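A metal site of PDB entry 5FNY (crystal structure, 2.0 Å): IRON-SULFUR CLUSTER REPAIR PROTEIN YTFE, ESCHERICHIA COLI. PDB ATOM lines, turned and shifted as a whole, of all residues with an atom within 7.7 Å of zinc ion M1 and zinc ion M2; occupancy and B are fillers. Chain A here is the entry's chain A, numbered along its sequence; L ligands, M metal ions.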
ATOM      1  N   ILE A  79      15.538  23.936 -10.172  1.00  0.00           N
ATOM      2  CA  ILE A  79      14.372  23.270  -9.593  1.00  0.00           C
ATOM      3  C   ILE A  79      13.759  22.283 -10.577  1.00  0.00           C
ATOM      4  O   ILE A  79      13.486  21.126 -10.215  1.00  0.00           O
ATOM      5  CB  ILE A  79      13.336  24.281  -9.115  1.00  0.00           C
ATOM      6  CG1 ILE A  79      13.847  24.985  -7.860  1.00  0.00           C
ATOM      7  CG2 ILE A  79      11.982  23.602  -8.837  1.00  0.00           C
ATOM      8  CD1 ILE A  79      13.065  26.213  -7.467  1.00  0.00           C
ATOM      9  N   ILE A  80      13.562  22.734 -11.815  1.00  0.00           N
ATOM     10  CA  ILE A  80      12.913  21.924 -12.840  1.00  0.00           C
ATOM     11  C   ILE A  80      13.712  20.645 -13.127  1.00  0.00           C
ATOM     12  O   ILE A  80      13.130  19.552 -13.142  1.00  0.00           O
ATOM     13  CB  ILE A  80      12.639  22.725 -14.123  1.00  0.00           C
ATOM     14  CG1 ILE A  80      11.606  23.818 -13.840  1.00  0.00           C
ATOM     15  CG2 ILE A  80      12.114  21.811 -15.214  1.00  0.00           C
ATOM     16  CD1 ILE A  80      11.499  24.867 -14.917  1.00  0.00           C
ATOM     17  N   TYR A  83      14.827  18.680  -9.245  1.00  0.00           N
ATOM     18  CA  TYR A  83      13.710  18.303  -8.407  1.00  0.00           C
ATOM     19  C   TYR A  83      12.439  17.887  -9.169  1.00  0.00           C
ATOM     20  O   TYR A  83      12.049  16.717  -9.067  1.00  0.00           O
ATOM     21  CB  TYR A  83      13.425  19.378  -7.370  1.00  0.00           C
ATOM     22  CG  TYR A  83      14.606  19.576  -6.426  1.00  0.00           C
ATOM     23  CD1 TYR A  83      15.099  18.514  -5.636  1.00  0.00           C
ATOM     24  CD2 TYR A  83      15.251  20.803  -6.323  1.00  0.00           C
ATOM     25  CE1 TYR A  83      16.158  18.676  -4.773  1.00  0.00           C
ATOM     26  CE2 TYR A  83      16.337  20.978  -5.458  1.00  0.00           C
ATOM     27  CZ  TYR A  83      16.797  19.902  -4.713  1.00  0.00           C
ATOM     28  OH  TYR A  83      17.871  20.080  -3.860  1.00  0.00           O
ATOM     29  N   HIS A  84      11.832  18.789  -9.946  1.00  0.00           N
ATOM     30  CA  HIS A  84      10.573  18.465 -10.640  1.00  0.00           C
ATOM     31  C   HIS A  84      10.691  17.193 -11.491  1.00  0.00           C
ATOM     32  O   HIS A  84       9.921  16.251 -11.331  1.00  0.00           O
ATOM     33  CB  HIS A  84      10.060  19.619 -11.515  1.00  0.00           C
ATOM     34  CG  HIS A  84       9.511  20.774 -10.726  1.00  0.00           C
ATOM     35  ND1 HIS A  84       8.675  21.702 -11.285  1.00  0.00           N
ATOM     36  CD2 HIS A  84       9.632  21.120  -9.428  1.00  0.00           C
ATOM     37  CE1 HIS A  84       8.322  22.589 -10.370  1.00  0.00           C
ATOM     38  NE2 HIS A  84       8.878  22.263  -9.223  1.00  0.00           N
ATOM     39  N   HIS A  87      11.286  14.024  -9.325  1.00  0.00           N
ATOM     40  CA  HIS A  87      10.044  13.501  -8.745  1.00  0.00           C
ATOM     41  C   HIS A  87       9.169  12.739  -9.744  1.00  0.00           C
ATOM     42  O   HIS A  87       8.572  11.748  -9.379  1.00  0.00           O
ATOM     43  CB  HIS A  87       9.199  14.613  -8.183  1.00  0.00           C
ATOM     44  CG  HIS A  87       9.853  15.381  -7.086  1.00  0.00           C
ATOM     45  ND1 HIS A  87      10.782  14.818  -6.248  1.00  0.00           N
ATOM     46  CD2 HIS A  87       9.676  16.657  -6.669  1.00  0.00           C
ATOM     47  CE1 HIS A  87      11.188  15.729  -5.381  1.00  0.00           C
ATOM     48  NE2 HIS A  87      10.536  16.847  -5.606  1.00  0.00           N
ATOM     49  N   LEU A 126       1.374  16.524  -6.757  1.00  0.00           N
ATOM     50  CA  LEU A 126       2.629  17.056  -7.261  1.00  0.00           C
ATOM     51  C   LEU A 126       2.601  17.364  -8.750  1.00  0.00           C
ATOM     52  O   LEU A 126       3.083  18.404  -9.148  1.00  0.00           O
ATOM     53  CB  LEU A 126       3.803  16.096  -6.974  1.00  0.00           C
ATOM     54  CG  LEU A 126       4.499  16.232  -5.628  1.00  0.00           C
ATOM     55  CD1 LEU A 126       5.654  15.230  -5.595  1.00  0.00           C
ATOM     56  CD2 LEU A 126       5.016  17.651  -5.424  1.00  0.00           C
ATOM     57  N   HIS A 129       0.569  20.524  -9.366  1.00  0.00           N
ATOM     58  CA  HIS A 129       1.324  21.627  -8.763  1.00  0.00           C
ATOM     59  C   HIS A 129       2.531  22.076  -9.615  1.00  0.00           C
ATOM     60  O   HIS A 129       2.710  23.267  -9.886  1.00  0.00           O
ATOM     61  CB  HIS A 129       1.793  21.214  -7.387  1.00  0.00           C
ATOM     62  CG  HIS A 129       2.644  22.233  -6.718  1.00  0.00           C
ATOM     63  ND1 HIS A 129       2.120  23.282  -6.002  1.00  0.00           N
ATOM     64  CD2 HIS A 129       3.983  22.352  -6.654  1.00  0.00           C
ATOM     65  CE1 HIS A 129       3.115  24.014  -5.527  1.00  0.00           C
ATOM     66  NE2 HIS A 129       4.257  23.477  -5.922  1.00  0.00           N
ATOM     67  N   MET A 130       3.320  21.107 -10.050  1.00  0.00           N
ATOM     68  CA  MET A 130       4.525  21.405 -10.806  1.00  0.00           C
ATOM     69  C   MET A 130       4.196  21.985 -12.184  1.00  0.00           C
ATOM     70  O   MET A 130       4.963  22.778 -12.727  1.00  0.00           O
ATOM     71  CB  MET A 130       5.408  20.151 -10.949  1.00  0.00           C
ATOM     72  CG  MET A 130       6.010  19.691  -9.643  1.00  0.00           C
ATOM     73  SD  MET A 130       7.122  18.244  -9.709  1.00  0.00           S
ATOM     74  CE  MET A 130       6.189  17.012 -10.605  1.00  0.00           C
ATOM     75  N   GLU A 133       3.388  25.721 -11.734  1.00  0.00           N
ATOM     76  CA  GLU A 133       4.660  26.411 -11.550  1.00  0.00           C
ATOM     77  C   GLU A 133       5.326  26.586 -12.889  1.00  0.00           C
ATOM     78  O   GLU A 133       5.616  27.713 -13.275  1.00  0.00           O
ATOM     79  CB  GLU A 133       5.593  25.691 -10.567  1.00  0.00           C
ATOM     80  CG  GLU A 133       5.300  26.065  -9.136  1.00  0.00           C
ATOM     81  CD  GLU A 133       6.122  25.285  -8.092  1.00  0.00           C
ATOM     82  OE1 GLU A 133       6.830  24.300  -8.436  1.00  0.00           O
ATOM     83  OE2 GLU A 133       5.999  25.630  -6.908  1.00  0.00           O
ATOM     84  N   GLU A 134       5.549  25.483 -13.602  1.00  0.00           N
ATOM     85  CA  GLU A 134       6.350  25.524 -14.844  1.00  0.00           C
ATOM     86  C   GLU A 134       5.673  26.336 -15.953  1.00  0.00           C
ATOM     87  O   GLU A 134       6.331  27.075 -16.658  1.00  0.00           O
ATOM     88  CB  GLU A 134       6.678  24.103 -15.331  1.00  0.00           C
ATOM     89  CG  GLU A 134       7.686  23.386 -14.437  1.00  0.00           C
ATOM     90  CD  GLU A 134       7.860  21.899 -14.757  1.00  0.00           C
ATOM     91  OE1 GLU A 134       7.619  21.465 -15.900  1.00  0.00           O
ATOM     92  OE2 GLU A 134       8.269  21.134 -13.845  1.00  0.00           O
ATOM     93  N   LEU A 137       3.443  30.310 -13.216  1.00  0.00           N
ATOM     94  CA  LEU A 137       4.124  31.105 -12.224  1.00  0.00           C
ATOM     95  C   LEU A 137       5.629  31.328 -12.495  1.00  0.00           C
ATOM     96  O   LEU A 137       6.107  32.470 -12.430  1.00  0.00           O
ATOM     97  CB  LEU A 137       3.930  30.503 -10.819  1.00  0.00           C
ATOM     98  CG  LEU A 137       4.544  31.290  -9.673  1.00  0.00           C
ATOM     99  CD1 LEU A 137       3.992  32.696  -9.589  1.00  0.00           C
ATOM    100  CD2 LEU A 137       4.372  30.551  -8.354  1.00  0.00           C
ATOM    101  N   PHE A 138       6.374  30.280 -12.793  1.00  0.00           N
ATOM    102  CA  PHE A 138       7.834  30.454 -13.020  1.00  0.00           C
ATOM    103  C   PHE A 138       8.169  31.422 -14.189  1.00  0.00           C
ATOM    104  O   PHE A 138       9.088  32.231 -14.076  1.00  0.00           O
ATOM    105  CB  PHE A 138       8.567  29.115 -13.225  1.00  0.00           C
ATOM    106  CG  PHE A 138       8.739  28.258 -11.983  1.00  0.00           C
ATOM    107  CD1 PHE A 138       8.475  28.725 -10.680  1.00  0.00           C
ATOM    108  CD2 PHE A 138       9.260  26.958 -12.114  1.00  0.00           C
ATOM    109  CE1 PHE A 138       8.698  27.908  -9.568  1.00  0.00           C
ATOM    110  CE2 PHE A 138       9.478  26.158 -11.002  1.00  0.00           C
ATOM    111  CZ  PHE A 138       9.203  26.634  -9.733  1.00  0.00           C
ATOM    112  N   MET A 156       0.609  28.600  -3.876  1.00  0.00           N
ATOM    113  CA  MET A 156       1.622  27.577  -4.022  1.00  0.00           C
ATOM    114  C   MET A 156       2.178  27.139  -2.652  1.00  0.00           C
ATOM    115  O   MET A 156       2.459  25.961  -2.442  1.00  0.00           O
ATOM    116  CB  MET A 156       2.763  28.063  -4.908  1.00  0.00           C
ATOM    117  CG  MET A 156       2.361  28.386  -6.334  1.00  0.00           C
ATOM    118  SD  MET A 156       1.725  26.987  -7.279  1.00  0.00           S
ATOM    119  CE  MET A 156      -0.035  27.135  -7.071  1.00  0.00           C
ATOM    120  N   GLU A 157       2.333  28.080  -1.727  1.00  0.00           N
ATOM    121  CA  GLU A 157       2.830  27.706  -0.407  1.00  0.00           C
ATOM    122  C   GLU A 157       1.802  26.882   0.355  1.00  0.00           C
ATOM    123  O   GLU A 157       2.171  25.984   1.118  1.00  0.00           O
ATOM    124  CB  GLU A 157       3.305  28.941   0.379  1.00  0.00           C
ATOM    125  CG  GLU A 157       4.499  29.597  -0.283  1.00  0.00           C
ATOM    126  CD  GLU A 157       5.226  30.610   0.598  1.00  0.00           C
ATOM    127  OE1 GLU A 157       4.605  31.188   1.516  1.00  0.00           O
ATOM    128  OE2 GLU A 157       6.438  30.851   0.342  1.00  0.00           O
ATOM    129  N   GLU A 159      -0.213  24.766  -1.151  1.00  0.00           N
ATOM    130  CA  GLU A 159      -0.037  23.452  -1.774  1.00  0.00           C
ATOM    131  C   GLU A 159       1.219  22.706  -1.260  1.00  0.00           C
ATOM    132  O   GLU A 159       1.173  21.491  -1.052  1.00  0.00           O
ATOM    133  CB  GLU A 159      -0.028  23.586  -3.301  1.00  0.00           C
ATOM    134  CG  GLU A 159      -1.405  24.003  -3.855  1.00  0.00           C
ATOM    135  CD  GLU A 159      -1.523  23.973  -5.374  1.00  0.00           C
ATOM    136  OE1 GLU A 159      -0.534  23.658  -6.087  1.00  0.00           O
ATOM    137  OE2 GLU A 159      -2.623  24.276  -5.882  1.00  0.00           O
ATOM    138  N   HIS A 160       2.307  23.424  -1.006  1.00  0.00           N
ATOM    139  CA  HIS A 160       3.458  22.820  -0.322  1.00  0.00           C
ATOM    140  C   HIS A 160       3.107  22.243   1.050  1.00  0.00           C
ATOM    141  O   HIS A 160       3.551  21.128   1.398  1.00  0.00           O
ATOM    142  CB  HIS A 160       4.575  23.846  -0.157  1.00  0.00           C
ATOM    143  CG  HIS A 160       5.170  24.270  -1.454  1.00  0.00           C
ATOM    144  ND1 HIS A 160       6.013  25.356  -1.557  1.00  0.00           N
ATOM    145  CD2 HIS A 160       5.026  23.792  -2.711  1.00  0.00           C
ATOM    146  CE1 HIS A 160       6.395  25.491  -2.810  1.00  0.00           C
ATOM    147  NE2 HIS A 160       5.810  24.566  -3.535  1.00  0.00           N
ATOM    148  N   LEU A 201      12.148  16.275  -1.666  1.00  0.00           N
ATOM    149  CA  LEU A 201      10.960  17.100  -1.606  1.00  0.00           C
ATOM    150  C   LEU A 201      11.132  18.229  -0.609  1.00  0.00           C
ATOM    151  O   LEU A 201      10.700  19.368  -0.866  1.00  0.00           O
ATOM    152  CB  LEU A 201       9.746  16.219  -1.316  1.00  0.00           C
ATOM    153  CG  LEU A 201       8.353  16.699  -1.619  1.00  0.00           C
ATOM    154  CD1 LEU A 201       8.243  17.507  -2.905  1.00  0.00           C
ATOM    155  CD2 LEU A 201       7.447  15.475  -1.661  1.00  0.00           C
ATOM    156  N   HIS A 204      13.623  20.718  -2.176  1.00  0.00           N
ATOM    157  CA  HIS A 204      12.857  21.393  -3.234  1.00  0.00           C
ATOM    158  C   HIS A 204      11.950  22.471  -2.633  1.00  0.00           C
ATOM    159  O   HIS A 204      12.044  23.648  -3.013  1.00  0.00           O
ATOM    160  CB  HIS A 204      12.093  20.304  -4.015  1.00  0.00           C
ATOM    161  CG  HIS A 204      11.022  20.791  -4.959  1.00  0.00           C
ATOM    162  ND1 HIS A 204      10.070  19.921  -5.452  1.00  0.00           N
ATOM    163  CD2 HIS A 204      10.745  21.994  -5.520  1.00  0.00           C
ATOM    164  CE1 HIS A 204       9.230  20.577  -6.219  1.00  0.00           C
ATOM    165  NE2 HIS A 204       9.622  21.832  -6.301  1.00  0.00           N
ATOM    166  N   ILE A 205      11.115  22.087  -1.694  1.00  0.00           N
ATOM    167  CA  ILE A 205      10.180  23.038  -1.102  1.00  0.00           C
ATOM    168  C   ILE A 205      10.968  24.116  -0.352  1.00  0.00           C
ATOM    169  O   ILE A 205      10.569  25.308  -0.359  1.00  0.00           O
ATOM    170  CB  ILE A 205       9.164  22.351  -0.166  1.00  0.00           C
ATOM    171  CG1 ILE A 205       8.276  21.312  -0.887  1.00  0.00           C
ATOM    172  CG2 ILE A 205       8.349  23.371   0.629  1.00  0.00           C
ATOM    173  CD1 ILE A 205       7.706  21.744  -2.197  1.00  0.00           C
ATOM    174  N   GLU A 208      12.154  26.749  -2.752  1.00  0.00           N
ATOM    175  CA  GLU A 208      11.054  27.618  -3.184  1.00  0.00           C
ATOM    176  C   GLU A 208      10.602  28.565  -2.063  1.00  0.00           C
ATOM    177  O   GLU A 208      10.566  29.788  -2.266  1.00  0.00           O
ATOM    178  CB  GLU A 208       9.910  26.784  -3.749  1.00  0.00           C
ATOM    179  CG  GLU A 208      10.307  26.065  -5.032  1.00  0.00           C
ATOM    180  CD  GLU A 208       9.211  25.245  -5.683  1.00  0.00           C
ATOM    181  OE1 GLU A 208       8.092  25.195  -5.137  1.00  0.00           O
ATOM    182  OE2 GLU A 208       9.464  24.676  -6.782  1.00  0.00           O
ATOM    183  N   ASN A 209      10.309  28.012  -0.886  1.00  0.00           N
ATOM    184  CA  ASN A 209       9.770  28.781   0.252  1.00  0.00           C
ATOM    185  C   ASN A 209      10.732  29.721   0.928  1.00  0.00           C
ATOM    186  O   ASN A 209      10.327  30.770   1.411  1.00  0.00           O
ATOM    187  CB  ASN A 209       9.205  27.862   1.340  1.00  0.00           C
ATOM    188  CG  ASN A 209       7.823  27.314   0.990  1.00  0.00           C
ATOM    189  OD1 ASN A 209       7.350  27.422  -0.128  1.00  0.00           O
ATOM    190  ND2 ASN A 209       7.182  26.717   1.969  1.00  0.00           N
ATOM    191  N   LEU A 212      13.364  31.330  -3.447  1.00  0.00           N
ATOM    192  CA  LEU A 212      12.748  31.808  -4.673  1.00  0.00           C
ATOM    193  C   LEU A 212      11.564  32.744  -4.422  1.00  0.00           C
ATOM    194  O   LEU A 212      11.555  33.873  -4.943  1.00  0.00           O
ATOM    195  CB  LEU A 212      12.291  30.657  -5.556  1.00  0.00           C
ATOM    196  CG  LEU A 212      11.724  31.038  -6.937  1.00  0.00           C
ATOM    197  CD1 LEU A 212      12.775  31.669  -7.849  1.00  0.00           C
ATOM    198  CD2 LEU A 212      11.080  29.823  -7.591  1.00  0.00           C
ATOM    199  N   PHE A 213      10.603  32.289  -3.649  1.00  0.00           N
ATOM    200  CA  PHE A 213       9.407  33.084  -3.415  1.00  0.00           C
ATOM    201  C   PHE A 213       9.651  34.366  -2.632  1.00  0.00           C
ATOM    202  O   PHE A 213       9.139  35.405  -3.033  1.00  0.00           O
ATOM    203  CB  PHE A 213       8.294  32.275  -2.762  1.00  0.00           C
ATOM    204  CG  PHE A 213       7.752  31.150  -3.626  1.00  0.00           C
ATOM    205  CD1 PHE A 213       7.981  31.069  -5.003  1.00  0.00           C
ATOM    206  CD2 PHE A 213       6.982  30.157  -3.028  1.00  0.00           C
ATOM    207  CE1 PHE A 213       7.464  30.019  -5.743  1.00  0.00           C
ATOM    208  CE2 PHE A 213       6.453  29.134  -3.774  1.00  0.00           C
ATOM    209  CZ  PHE A 213       6.713  29.043  -5.127  1.00  0.00           C
HETATM  210  O1  LIG L   1       6.983  22.704  -6.248  1.00  0.00           O
HETATM  211 ZN    ZN M   1       8.439  23.128  -7.408  1.00  0.00          ZN
HETATM  212 ZN    ZN M   2       6.132  24.229  -5.543  1.00  0.00          ZN
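Zinc ion M2 is bound by O1 of the ligand (1.9 Å), OE2 of Glu 133 (2.0 Å), NE2 of His 129 (2.1 Å), NE2 of His 160 (2.1 Å) and OE1 of Glu 208 (2.2 Å).
The backbone carbonyl oxygen (O) of Glu 208 sits at hydrogen-bond distance from the backbone NH (N) of Phe 213 (2.9 Å).
The backbone NH of Phe 138 is in hydrogen-bond range of the backbone carbonyl oxygen of Glu 133.
OE1 of Glu 159 lies within hydrogen-bond range of ND1 of His 129.
N of His 84 lies within hydrogen-bond range of O of Ile 79 (2.9 Å).
ND1 of His 84 lies within hydrogen-bond range of OE2 of Glu 134, at 2.7 Å.
The side-chain amide oxygen (OD1) of Asn 209 is in hydrogen-bond range of a ring nitrogen (ND1) of His 160 (2.8 Å).
A ring nitrogen (NE2) of His 87 is in hydrogen-bond range of a ring nitrogen (ND1) of His 204.
Zinc ion M1 is bound by O1 of the ligand, 1.9 Å away.
Zinc ion M1 is bound by OE2 of Glu 208.
Zinc ion M1 is bound by NE2 of His 84 (2.1 Å).
Zinc ion M1 is bound by NE2 of His 204 (2.1 Å).
OE1 of Glu 133 is bound to zinc ion M1 (2.2 Å).
Zinc ion M1 has five donor atoms within binding distance.
Ile 79 touches zinc ion M1 (CG2 to ZN, 3.8 Å).
Within 4 Å of zinc ion M1: Ile 79, His 84, Glu 133, His 204 and Glu 208.
Four residues have an atom within 4 Å of zinc ion M2: His 129, Glu 133, His 160 and Glu 208.
The nearest printed residue that does not touch zinc ion M2 is His 204 (4.3 Å).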
